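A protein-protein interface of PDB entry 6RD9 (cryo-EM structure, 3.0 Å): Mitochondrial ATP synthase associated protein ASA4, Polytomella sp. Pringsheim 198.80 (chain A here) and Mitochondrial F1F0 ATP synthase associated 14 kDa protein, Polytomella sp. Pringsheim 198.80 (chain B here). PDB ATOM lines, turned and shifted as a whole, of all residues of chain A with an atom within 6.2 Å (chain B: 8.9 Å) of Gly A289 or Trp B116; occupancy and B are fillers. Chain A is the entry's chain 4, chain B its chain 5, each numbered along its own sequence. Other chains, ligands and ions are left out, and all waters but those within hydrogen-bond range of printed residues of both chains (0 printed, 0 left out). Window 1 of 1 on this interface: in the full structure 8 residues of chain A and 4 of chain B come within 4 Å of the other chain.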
ATOM      1  N   PHE A 278      18.154  28.363 -24.815  1.00  0.00           N
ATOM      2  CA  PHE A 278      19.611  28.387 -24.886  1.00  0.00           C
ATOM      3  C   PHE A 278      20.164  29.654 -24.271  1.00  0.00           C
ATOM      4  O   PHE A 278      21.202  29.628 -23.609  1.00  0.00           O
ATOM      5  CB  PHE A 278      20.068  28.267 -26.337  1.00  0.00           C
ATOM      6  CG  PHE A 278      21.505  27.886 -26.494  1.00  0.00           C
ATOM      7  CD1 PHE A 278      22.502  28.846 -26.523  1.00  0.00           C
ATOM      8  CD2 PHE A 278      21.859  26.574 -26.642  1.00  0.00           C
ATOM      9  CE1 PHE A 278      23.804  28.498 -26.670  1.00  0.00           C
ATOM     10  CE2 PHE A 278      23.168  26.230 -26.790  1.00  0.00           C
ATOM     11  CZ  PHE A 278      24.137  27.194 -26.808  1.00  0.00           C
ATOM     12  N   SER A 281      19.512  29.145 -20.420  1.00  0.00           N
ATOM     13  CA  SER A 281      20.374  28.154 -19.797  1.00  0.00           C
ATOM     14  C   SER A 281      21.816  28.606 -19.710  1.00  0.00           C
ATOM     15  O   SER A 281      22.553  28.106 -18.864  1.00  0.00           O
ATOM     16  CB  SER A 281      20.312  26.846 -20.565  1.00  0.00           C
ATOM     17  OG  SER A 281      21.195  25.907 -20.006  1.00  0.00           O
ATOM     18  N   VAL A 282      22.240  29.517 -20.577  1.00  0.00           N
ATOM     19  CA  VAL A 282      23.590  30.054 -20.497  1.00  0.00           C
ATOM     20  C   VAL A 282      23.669  31.111 -19.414  1.00  0.00           C
ATOM     21  O   VAL A 282      24.663  31.188 -18.685  1.00  0.00           O
ATOM     22  CB  VAL A 282      24.001  30.577 -21.881  1.00  0.00           C
ATOM     23  CG1 VAL A 282      25.148  31.544 -21.810  1.00  0.00           C
ATOM     24  CG2 VAL A 282      24.381  29.426 -22.746  1.00  0.00           C
ATOM     25  N   ALA A 283      22.599  31.883 -19.236  1.00  0.00           N
ATOM     26  CA  ALA A 283      22.528  32.883 -18.184  1.00  0.00           C
ATOM     27  C   ALA A 283      22.552  32.280 -16.790  1.00  0.00           C
ATOM     28  O   ALA A 283      22.925  32.969 -15.843  1.00  0.00           O
ATOM     29  CB  ALA A 283      21.265  33.712 -18.354  1.00  0.00           C
ATOM     30  N   ALA A 285      24.465  29.528 -15.900  1.00  0.00           N
ATOM     31  CA  ALA A 285      25.869  29.226 -15.627  1.00  0.00           C
ATOM     32  C   ALA A 285      26.682  29.433 -16.887  1.00  0.00           C
ATOM     33  O   ALA A 285      26.784  28.542 -17.733  1.00  0.00           O
ATOM     34  CB  ALA A 285      26.057  27.808 -15.096  1.00  0.00           C
ATOM     35  N   PRO A 286      27.300  30.602 -17.037  1.00  0.00           N
ATOM     36  CA  PRO A 286      27.985  30.913 -18.294  1.00  0.00           C
ATOM     37  C   PRO A 286      29.336  30.256 -18.464  1.00  0.00           C
ATOM     38  O   PRO A 286      29.781  30.099 -19.603  1.00  0.00           O
ATOM     39  CB  PRO A 286      28.121  32.427 -18.231  1.00  0.00           C
ATOM     40  CG  PRO A 286      27.158  32.849 -17.198  1.00  0.00           C
ATOM     41  CD  PRO A 286      27.138  31.800 -16.209  1.00  0.00           C
ATOM     42  N   ALA A 287      30.038  29.918 -17.396  1.00  0.00           N
ATOM     43  CA  ALA A 287      31.275  29.184 -17.589  1.00  0.00           C
ATOM     44  C   ALA A 287      31.030  27.717 -17.890  1.00  0.00           C
ATOM     45  O   ALA A 287      31.942  27.032 -18.361  1.00  0.00           O
ATOM     46  CB  ALA A 287      32.166  29.318 -16.362  1.00  0.00           C
ATOM     47  N   SER A 288      29.824  27.224 -17.626  1.00  0.00           N
ATOM     48  CA  SER A 288      29.430  25.859 -17.927  1.00  0.00           C
ATOM     49  C   SER A 288      28.877  25.723 -19.332  1.00  0.00           C
ATOM     50  O   SER A 288      29.253  24.803 -20.060  1.00  0.00           O
ATOM     51  CB  SER A 288      28.384  25.391 -16.919  1.00  0.00           C
ATOM     52  OG  SER A 288      27.772  24.187 -17.333  1.00  0.00           O
ATOM     53  N   GLY A 289      28.011  26.637 -19.734  1.00  0.00           N
ATOM     54  CA  GLY A 289      27.357  26.554 -21.010  1.00  0.00           C
ATOM     55  C   GLY A 289      25.898  26.215 -20.852  1.00  0.00           C
ATOM     56  O   GLY A 289      25.297  26.455 -19.805  1.00  0.00           O
ATOM     57  N   PRO A 290      25.291  25.667 -21.896  1.00  0.00           N
ATOM     58  CA  PRO A 290      23.927  25.162 -21.762  1.00  0.00           C
ATOM     59  C   PRO A 290      23.896  23.864 -20.976  1.00  0.00           C
ATOM     60  O   PRO A 290      24.864  23.105 -20.943  1.00  0.00           O
ATOM     61  CB  PRO A 290      23.494  24.943 -23.211  1.00  0.00           C
ATOM     62  CG  PRO A 290      24.741  24.713 -23.919  1.00  0.00           C
ATOM     63  CD  PRO A 290      25.757  25.590 -23.284  1.00  0.00           C
ATOM     64  N   LYS A 291      22.762  23.620 -20.330  1.00  0.00           N
ATOM     65  CA  LYS A 291      22.582  22.427 -19.518  1.00  0.00           C
ATOM     66  C   LYS A 291      22.068  21.292 -20.384  1.00  0.00           C
ATOM     67  O   LYS A 291      20.983  21.393 -20.954  1.00  0.00           O
ATOM     68  CB  LYS A 291      21.594  22.702 -18.390  1.00  0.00           C
ATOM     69  CG  LYS A 291      22.042  23.788 -17.471  1.00  0.00           C
ATOM     70  CD  LYS A 291      23.250  23.339 -16.682  1.00  0.00           C
ATOM     71  CE  LYS A 291      23.875  24.504 -15.943  1.00  0.00           C
ATOM     72  NZ  LYS A 291      24.542  25.401 -16.916  1.00  0.00           N
ATOM     73  N   ALA B 105      29.416  40.554 -24.415  1.00  0.00           N
ATOM     74  CA  ALA B 105      29.590  39.536 -25.419  1.00  0.00           C
ATOM     75  C   ALA B 105      30.832  38.703 -25.196  1.00  0.00           C
ATOM     76  O   ALA B 105      30.867  37.554 -25.622  1.00  0.00           O
ATOM     77  CB  ALA B 105      29.638  40.180 -26.779  1.00  0.00           C
ATOM     78  N   LEU B 108      33.295  35.682 -20.581  1.00  0.00           N
ATOM     79  CA  LEU B 108      33.159  34.328 -20.001  1.00  0.00           C
ATOM     80  C   LEU B 108      32.505  34.331 -18.634  1.00  0.00           C
ATOM     81  O   LEU B 108      32.233  33.263 -18.123  1.00  0.00           O
ATOM     82  CB  LEU B 108      34.456  33.517 -19.859  1.00  0.00           C
ATOM     83  CG  LEU B 108      35.139  33.246 -21.185  1.00  0.00           C
ATOM     84  CD1 LEU B 108      36.480  32.568 -20.985  1.00  0.00           C
ATOM     85  CD2 LEU B 108      34.221  32.413 -22.039  1.00  0.00           C
ATOM     86  N   GLN B 109      32.227  35.474 -18.039  1.00  0.00           N
ATOM     87  CA  GLN B 109      31.405  35.501 -16.846  1.00  0.00           C
ATOM     88  C   GLN B 109      30.129  36.279 -17.048  1.00  0.00           C
ATOM     89  O   GLN B 109      29.353  36.414 -16.104  1.00  0.00           O
ATOM     90  CB  GLN B 109      32.152  36.098 -15.652  1.00  0.00           C
ATOM     91  CG  GLN B 109      32.921  35.114 -14.810  1.00  0.00           C
ATOM     92  CD  GLN B 109      34.248  34.766 -15.399  1.00  0.00           C
ATOM     93  OE1 GLN B 109      34.525  33.607 -15.688  1.00  0.00           O
ATOM     94  NE2 GLN B 109      35.089  35.768 -15.580  1.00  0.00           N
ATOM     95  N   SER B 110      29.892  36.796 -18.238  1.00  0.00           N
ATOM     96  CA  SER B 110      28.699  37.565 -18.495  1.00  0.00           C
ATOM     97  C   SER B 110      27.495  36.656 -18.625  1.00  0.00           C
ATOM     98  O   SER B 110      27.612  35.487 -18.930  1.00  0.00           O
ATOM     99  CB  SER B 110      28.873  38.367 -19.762  1.00  0.00           C
ATOM    100  OG  SER B 110      27.661  38.981 -20.122  1.00  0.00           O
ATOM    101  N   LYS B 111      26.319  37.207 -18.414  1.00  0.00           N
ATOM    102  CA  LYS B 111      25.140  36.384 -18.595  1.00  0.00           C
ATOM    103  C   LYS B 111      24.782  36.209 -20.056  1.00  0.00           C
ATOM    104  O   LYS B 111      23.966  35.346 -20.373  1.00  0.00           O
ATOM    105  CB  LYS B 111      23.953  36.970 -17.845  1.00  0.00           C
ATOM    106  CG  LYS B 111      24.170  37.097 -16.359  1.00  0.00           C
ATOM    107  CD  LYS B 111      24.600  35.786 -15.747  1.00  0.00           C
ATOM    108  CE  LYS B 111      25.020  35.955 -14.300  1.00  0.00           C
ATOM    109  NZ  LYS B 111      25.635  34.719 -13.754  1.00  0.00           N
ATOM    110  N   ARG B 112      25.357  37.010 -20.957  1.00  0.00           N
ATOM    111  CA  ARG B 112      25.104  36.869 -22.387  1.00  0.00           C
ATOM    112  C   ARG B 112      26.415  36.794 -23.138  1.00  0.00           C
ATOM    113  O   ARG B 112      26.690  37.684 -23.923  1.00  0.00           O
ATOM    114  CB  ARG B 112      24.288  38.043 -22.880  1.00  0.00           C
ATOM    115  CG  ARG B 112      22.904  38.096 -22.324  1.00  0.00           C
ATOM    116  CD  ARG B 112      22.195  39.380 -22.639  1.00  0.00           C
ATOM    117  NE  ARG B 112      22.668  40.484 -21.824  1.00  0.00           N
ATOM    118  CZ  ARG B 112      23.107  41.632 -22.317  1.00  0.00           C
ATOM    119  NH1 ARG B 112      23.509  42.584 -21.497  1.00  0.00           N
ATOM    120  NH2 ARG B 112      23.124  41.833 -23.626  1.00  0.00           N
ATOM    121  N   VAL B 113      27.109  35.688 -23.060  1.00  0.00           N
ATOM    122  CA  VAL B 113      28.399  35.585 -23.722  1.00  0.00           C
ATOM    123  C   VAL B 113      28.126  35.074 -25.116  1.00  0.00           C
ATOM    124  O   VAL B 113      27.155  34.351 -25.338  1.00  0.00           O
ATOM    125  CB  VAL B 113      29.355  34.631 -22.994  1.00  0.00           C
ATOM    126  CG1 VAL B 113      30.773  34.974 -23.301  1.00  0.00           C
ATOM    127  CG2 VAL B 113      29.140  34.642 -21.597  1.00  0.00           C
ATOM    128  N   LEU B 114      28.969  35.434 -26.061  1.00  0.00           N
ATOM    129  CA  LEU B 114      28.827  34.845 -27.373  1.00  0.00           C
ATOM    130  C   LEU B 114      29.627  33.575 -27.541  1.00  0.00           C
ATOM    131  O   LEU B 114      29.702  33.083 -28.658  1.00  0.00           O
ATOM    132  CB  LEU B 114      29.248  35.826 -28.456  1.00  0.00           C
ATOM    133  CG  LEU B 114      28.493  37.133 -28.587  1.00  0.00           C
ATOM    134  CD1 LEU B 114      28.736  37.662 -29.953  1.00  0.00           C
ATOM    135  CD2 LEU B 114      27.022  36.979 -28.349  1.00  0.00           C
ATOM    136  N   ILE B 115      30.229  33.023 -26.491  1.00  0.00           N
ATOM    137  CA  ILE B 115      31.138  31.908 -26.706  1.00  0.00           C
ATOM    138  C   ILE B 115      30.388  30.618 -26.987  1.00  0.00           C
ATOM    139  O   ILE B 115      30.927  29.721 -27.630  1.00  0.00           O
ATOM    140  CB  ILE B 115      32.103  31.784 -25.513  1.00  0.00           C
ATOM    141  CG1 ILE B 115      33.280  30.879 -25.834  1.00  0.00           C
ATOM    142  CG2 ILE B 115      31.406  31.275 -24.300  1.00  0.00           C
ATOM    143  CD1 ILE B 115      34.107  31.380 -26.948  1.00  0.00           C
ATOM    144  N   TRP B 116      29.135  30.510 -26.586  1.00  0.00           N
ATOM    145  CA  TRP B 116      28.361  29.329 -26.902  1.00  0.00           C
ATOM    146  C   TRP B 116      27.551  29.525 -28.153  1.00  0.00           C
ATOM    147  O   TRP B 116      26.924  28.583 -28.628  1.00  0.00           O
ATOM    148  CB  TRP B 116      27.449  28.969 -25.737  1.00  0.00           C
ATOM    149  CG  TRP B 116      28.150  29.043 -24.455  1.00  0.00           C
ATOM    150  CD1 TRP B 116      27.972  29.964 -23.496  1.00  0.00           C
ATOM    151  CD2 TRP B 116      29.174  28.171 -23.994  1.00  0.00           C
ATOM    152  NE1 TRP B 116      28.814  29.730 -22.455  1.00  0.00           N
ATOM    153  CE2 TRP B 116      29.570  28.631 -22.742  1.00  0.00           C
ATOM    154  CE3 TRP B 116      29.797  27.044 -24.523  1.00  0.00           C
ATOM    155  CZ2 TRP B 116      30.546  28.005 -22.006  1.00  0.00           C
ATOM    156  CZ3 TRP B 116      30.769  26.433 -23.795  1.00  0.00           C
ATOM    157  CH2 TRP B 116      31.136  26.909 -22.552  1.00  0.00           C
ATOM    158  N   GLN B 117      27.550  30.728 -28.692  1.00  0.00           N
ATOM    159  CA  GLN B 117      26.909  30.979 -29.955  1.00  0.00           C
ATOM    160  C   GLN B 117      27.868  30.930 -31.115  1.00  0.00           C
ATOM    161  O   GLN B 117      27.429  30.672 -32.229  1.00  0.00           O
ATOM    162  CB  GLN B 117      26.249  32.348 -29.967  1.00  0.00           C
ATOM    163  CG  GLN B 117      25.532  32.705 -28.745  1.00  0.00           C
ATOM    164  CD  GLN B 117      24.743  33.943 -28.947  1.00  0.00           C
ATOM    165  OE1 GLN B 117      24.593  34.404 -30.060  1.00  0.00           O
ATOM    166  NE2 GLN B 117      24.240  34.505 -27.873  1.00  0.00           N
ATOM    167  N   VAL B 118      29.146  31.203 -30.905  1.00  0.00           N
ATOM    168  CA  VAL B 118      30.081  31.224 -32.013  1.00  0.00           C
ATOM    169  C   VAL B 118      30.943  29.980 -32.051  1.00  0.00           C
ATOM    170  O   VAL B 118      31.368  29.579 -33.141  1.00  0.00           O
ATOM    171  CB  VAL B 118      30.951  32.499 -32.006  1.00  0.00           C
ATOM    172  CG1 VAL B 118      30.093  33.705 -31.915  1.00  0.00           C
ATOM    173  CG2 VAL B 118      31.966  32.512 -30.931  1.00  0.00           C
ATOM    174  N   LYS B 119      31.168  29.326 -30.930  1.00  0.00           N
ATOM    175  CA  LYS B 119      31.934  28.094 -30.869  1.00  0.00           C
ATOM    176  C   LYS B 119      31.066  27.150 -30.068  1.00  0.00           C
ATOM    177  O   LYS B 119      31.176  27.101 -28.838  1.00  0.00           O
ATOM    178  CB  LYS B 119      33.285  28.302 -30.204  1.00  0.00           C
ATOM    179  CG  LYS B 119      34.317  28.926 -31.079  1.00  0.00           C
ATOM    180  CD  LYS B 119      34.824  27.945 -32.079  1.00  0.00           C
ATOM    181  CE  LYS B 119      35.811  28.593 -33.001  1.00  0.00           C
ATOM    182  NZ  LYS B 119      36.221  27.672 -34.087  1.00  0.00           N
ATOM    183  N   PRO B 120      30.179  26.409 -30.721  1.00  0.00           N
ATOM    184  CA  PRO B 120      29.263  25.546 -29.986  1.00  0.00           C
ATOM    185  C   PRO B 120      29.986  24.389 -29.327  1.00  0.00           C
ATOM    186  O   PRO B 120      30.928  23.821 -29.878  1.00  0.00           O
ATOM    187  CB  PRO B 120      28.299  25.064 -31.068  1.00  0.00           C
ATOM    188  CG  PRO B 120      29.001  25.228 -32.296  1.00  0.00           C
ATOM    189  CD  PRO B 120      29.872  26.404 -32.154  1.00  0.00           C
ATOM    190  N   ALA B 121      29.538  24.060 -28.126  1.00  0.00           N
ATOM    191  CA  ALA B 121      30.244  23.139 -27.259  1.00  0.00           C
ATOM    192  C   ALA B 121      30.066  21.709 -27.721  1.00  0.00           C
ATOM    193  O   ALA B 121      28.974  21.308 -28.111  1.00  0.00           O
ATOM    194  CB  ALA B 121      29.731  23.283 -25.836  1.00  0.00           C
ATOM    195  N   LEU B 122      31.135  20.936 -27.650  1.00  0.00           N
ATOM    196  CA  LEU B 122      31.072  19.515 -27.934  1.00  0.00           C
ATOM    197  C   LEU B 122      30.600  18.775 -26.699  1.00  0.00           C
ATOM    198  O   LEU B 122      31.312  18.714 -25.700  1.00  0.00           O
ATOM    199  CB  LEU B 122      32.437  19.007 -28.353  1.00  0.00           C
ATOM    200  CG  LEU B 122      32.707  19.130 -29.824  1.00  0.00           C
ATOM    201  CD1 LEU B 122      34.116  18.781 -30.106  1.00  0.00           C
ATOM    202  CD2 LEU B 122      31.827  18.168 -30.473  1.00  0.00           C
ATOM    203  N   PHE B 123      29.419  18.195 -26.764  1.00  0.00           N
ATOM    204  CA  PHE B 123      28.919  17.454 -25.629  1.00  0.00           C
ATOM    205  C   PHE B 123      28.942  15.954 -25.858  1.00  0.00           C
ATOM    206  O   PHE B 123      28.623  15.477 -26.941  1.00  0.00           O
ATOM    207  CB  PHE B 123      27.513  17.907 -25.298  1.00  0.00           C
ATOM    208  CG  PHE B 123      27.470  19.027 -24.339  1.00  0.00           C
ATOM    209  CD1 PHE B 123      27.468  18.783 -22.992  1.00  0.00           C
ATOM    210  CD2 PHE B 123      27.447  20.323 -24.773  1.00  0.00           C
ATOM    211  CE1 PHE B 123      27.430  19.816 -22.099  1.00  0.00           C
ATOM    212  CE2 PHE B 123      27.410  21.359 -23.883  1.00  0.00           C
ATOM    213  CZ  PHE B 123      27.404  21.103 -22.547  1.00  0.00           C
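Gly A289 touches one residue of chain B.
Trp B116 touches five residues of chain A.
Ser A288 touches just one residue of chain B: Trp B116.
Printed residues of chain B within 4 Å of Pro A290: Phe B123.
Of the printed residues of chain A, Lys B111 touches Ala A283 (3.3 Å).
Of the printed residues of chain A, Ser B110 touches Pro A286.
Of the printed residues of chain B, Ala A283 touches Lys B111 (3.3 Å).
Ala B121 touches none of the printed residues of chain A.
Val B118 touches none of the printed residues of chain A.
The nearest residue of chain B that does not touch Gly A289 is Phe B123 (5.6 Å).
The nearest residue of chain A that does not touch Trp B116 is Ala A287 (4.02 Å).
The nearest printed residue of chain A that does not touch Lys B111 is Pro A286 (4.1 Å).
NE1 of Trp B116 is in hydrogen-bond range of O of Pro A286 (3.0 Å).
The side-chain hydroxyl (OG) of Ser A288 is in hydrogen-bond range of the side-chain amino group (NZ) of Lys A291 (3.5 Å).
NZ of Lys A291 is in hydrogen-bond range of O of Gly A289.
OG of Ser B110 lies within hydrogen-bond range of N of Arg B112, at 3.1 Å.
Phe A278 touches Trp B116 (CZ to O, 3.6 Å).
CG1 of Val A282 touches CD1 of Trp B116, 3.6 Å away.
Lys B111 touches Ala A283 (CD to O, 3.3 Å).
Pro A286 touches Ser B110 (CB to O, 3.2 Å).
O of Ser A288 touches CH2 of Trp B116, 3.8 Å away.
Trp B116 touches Gly A289.
Pro A290 touches Phe B123 (O to CZ, 3.6 Å).
Of the 11 printed residues of chain A, 7 touch a printed residue of chain B.
Printed residues of chain A that touch a printed residue of chain B: Phe A278, Val A282, Ala A283, Pro A286, Ser A288, Gly A289 and Pro A290.
Hydrophobic or aromatic side chains of chain B within 4 Å of the printed part of chain A: Trp B116 and Phe B123.
Among the printed residues, no Asp or Glu carboxylate lies within 4 Å of a Lys or Arg side-chain nitrogen of the other chain.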
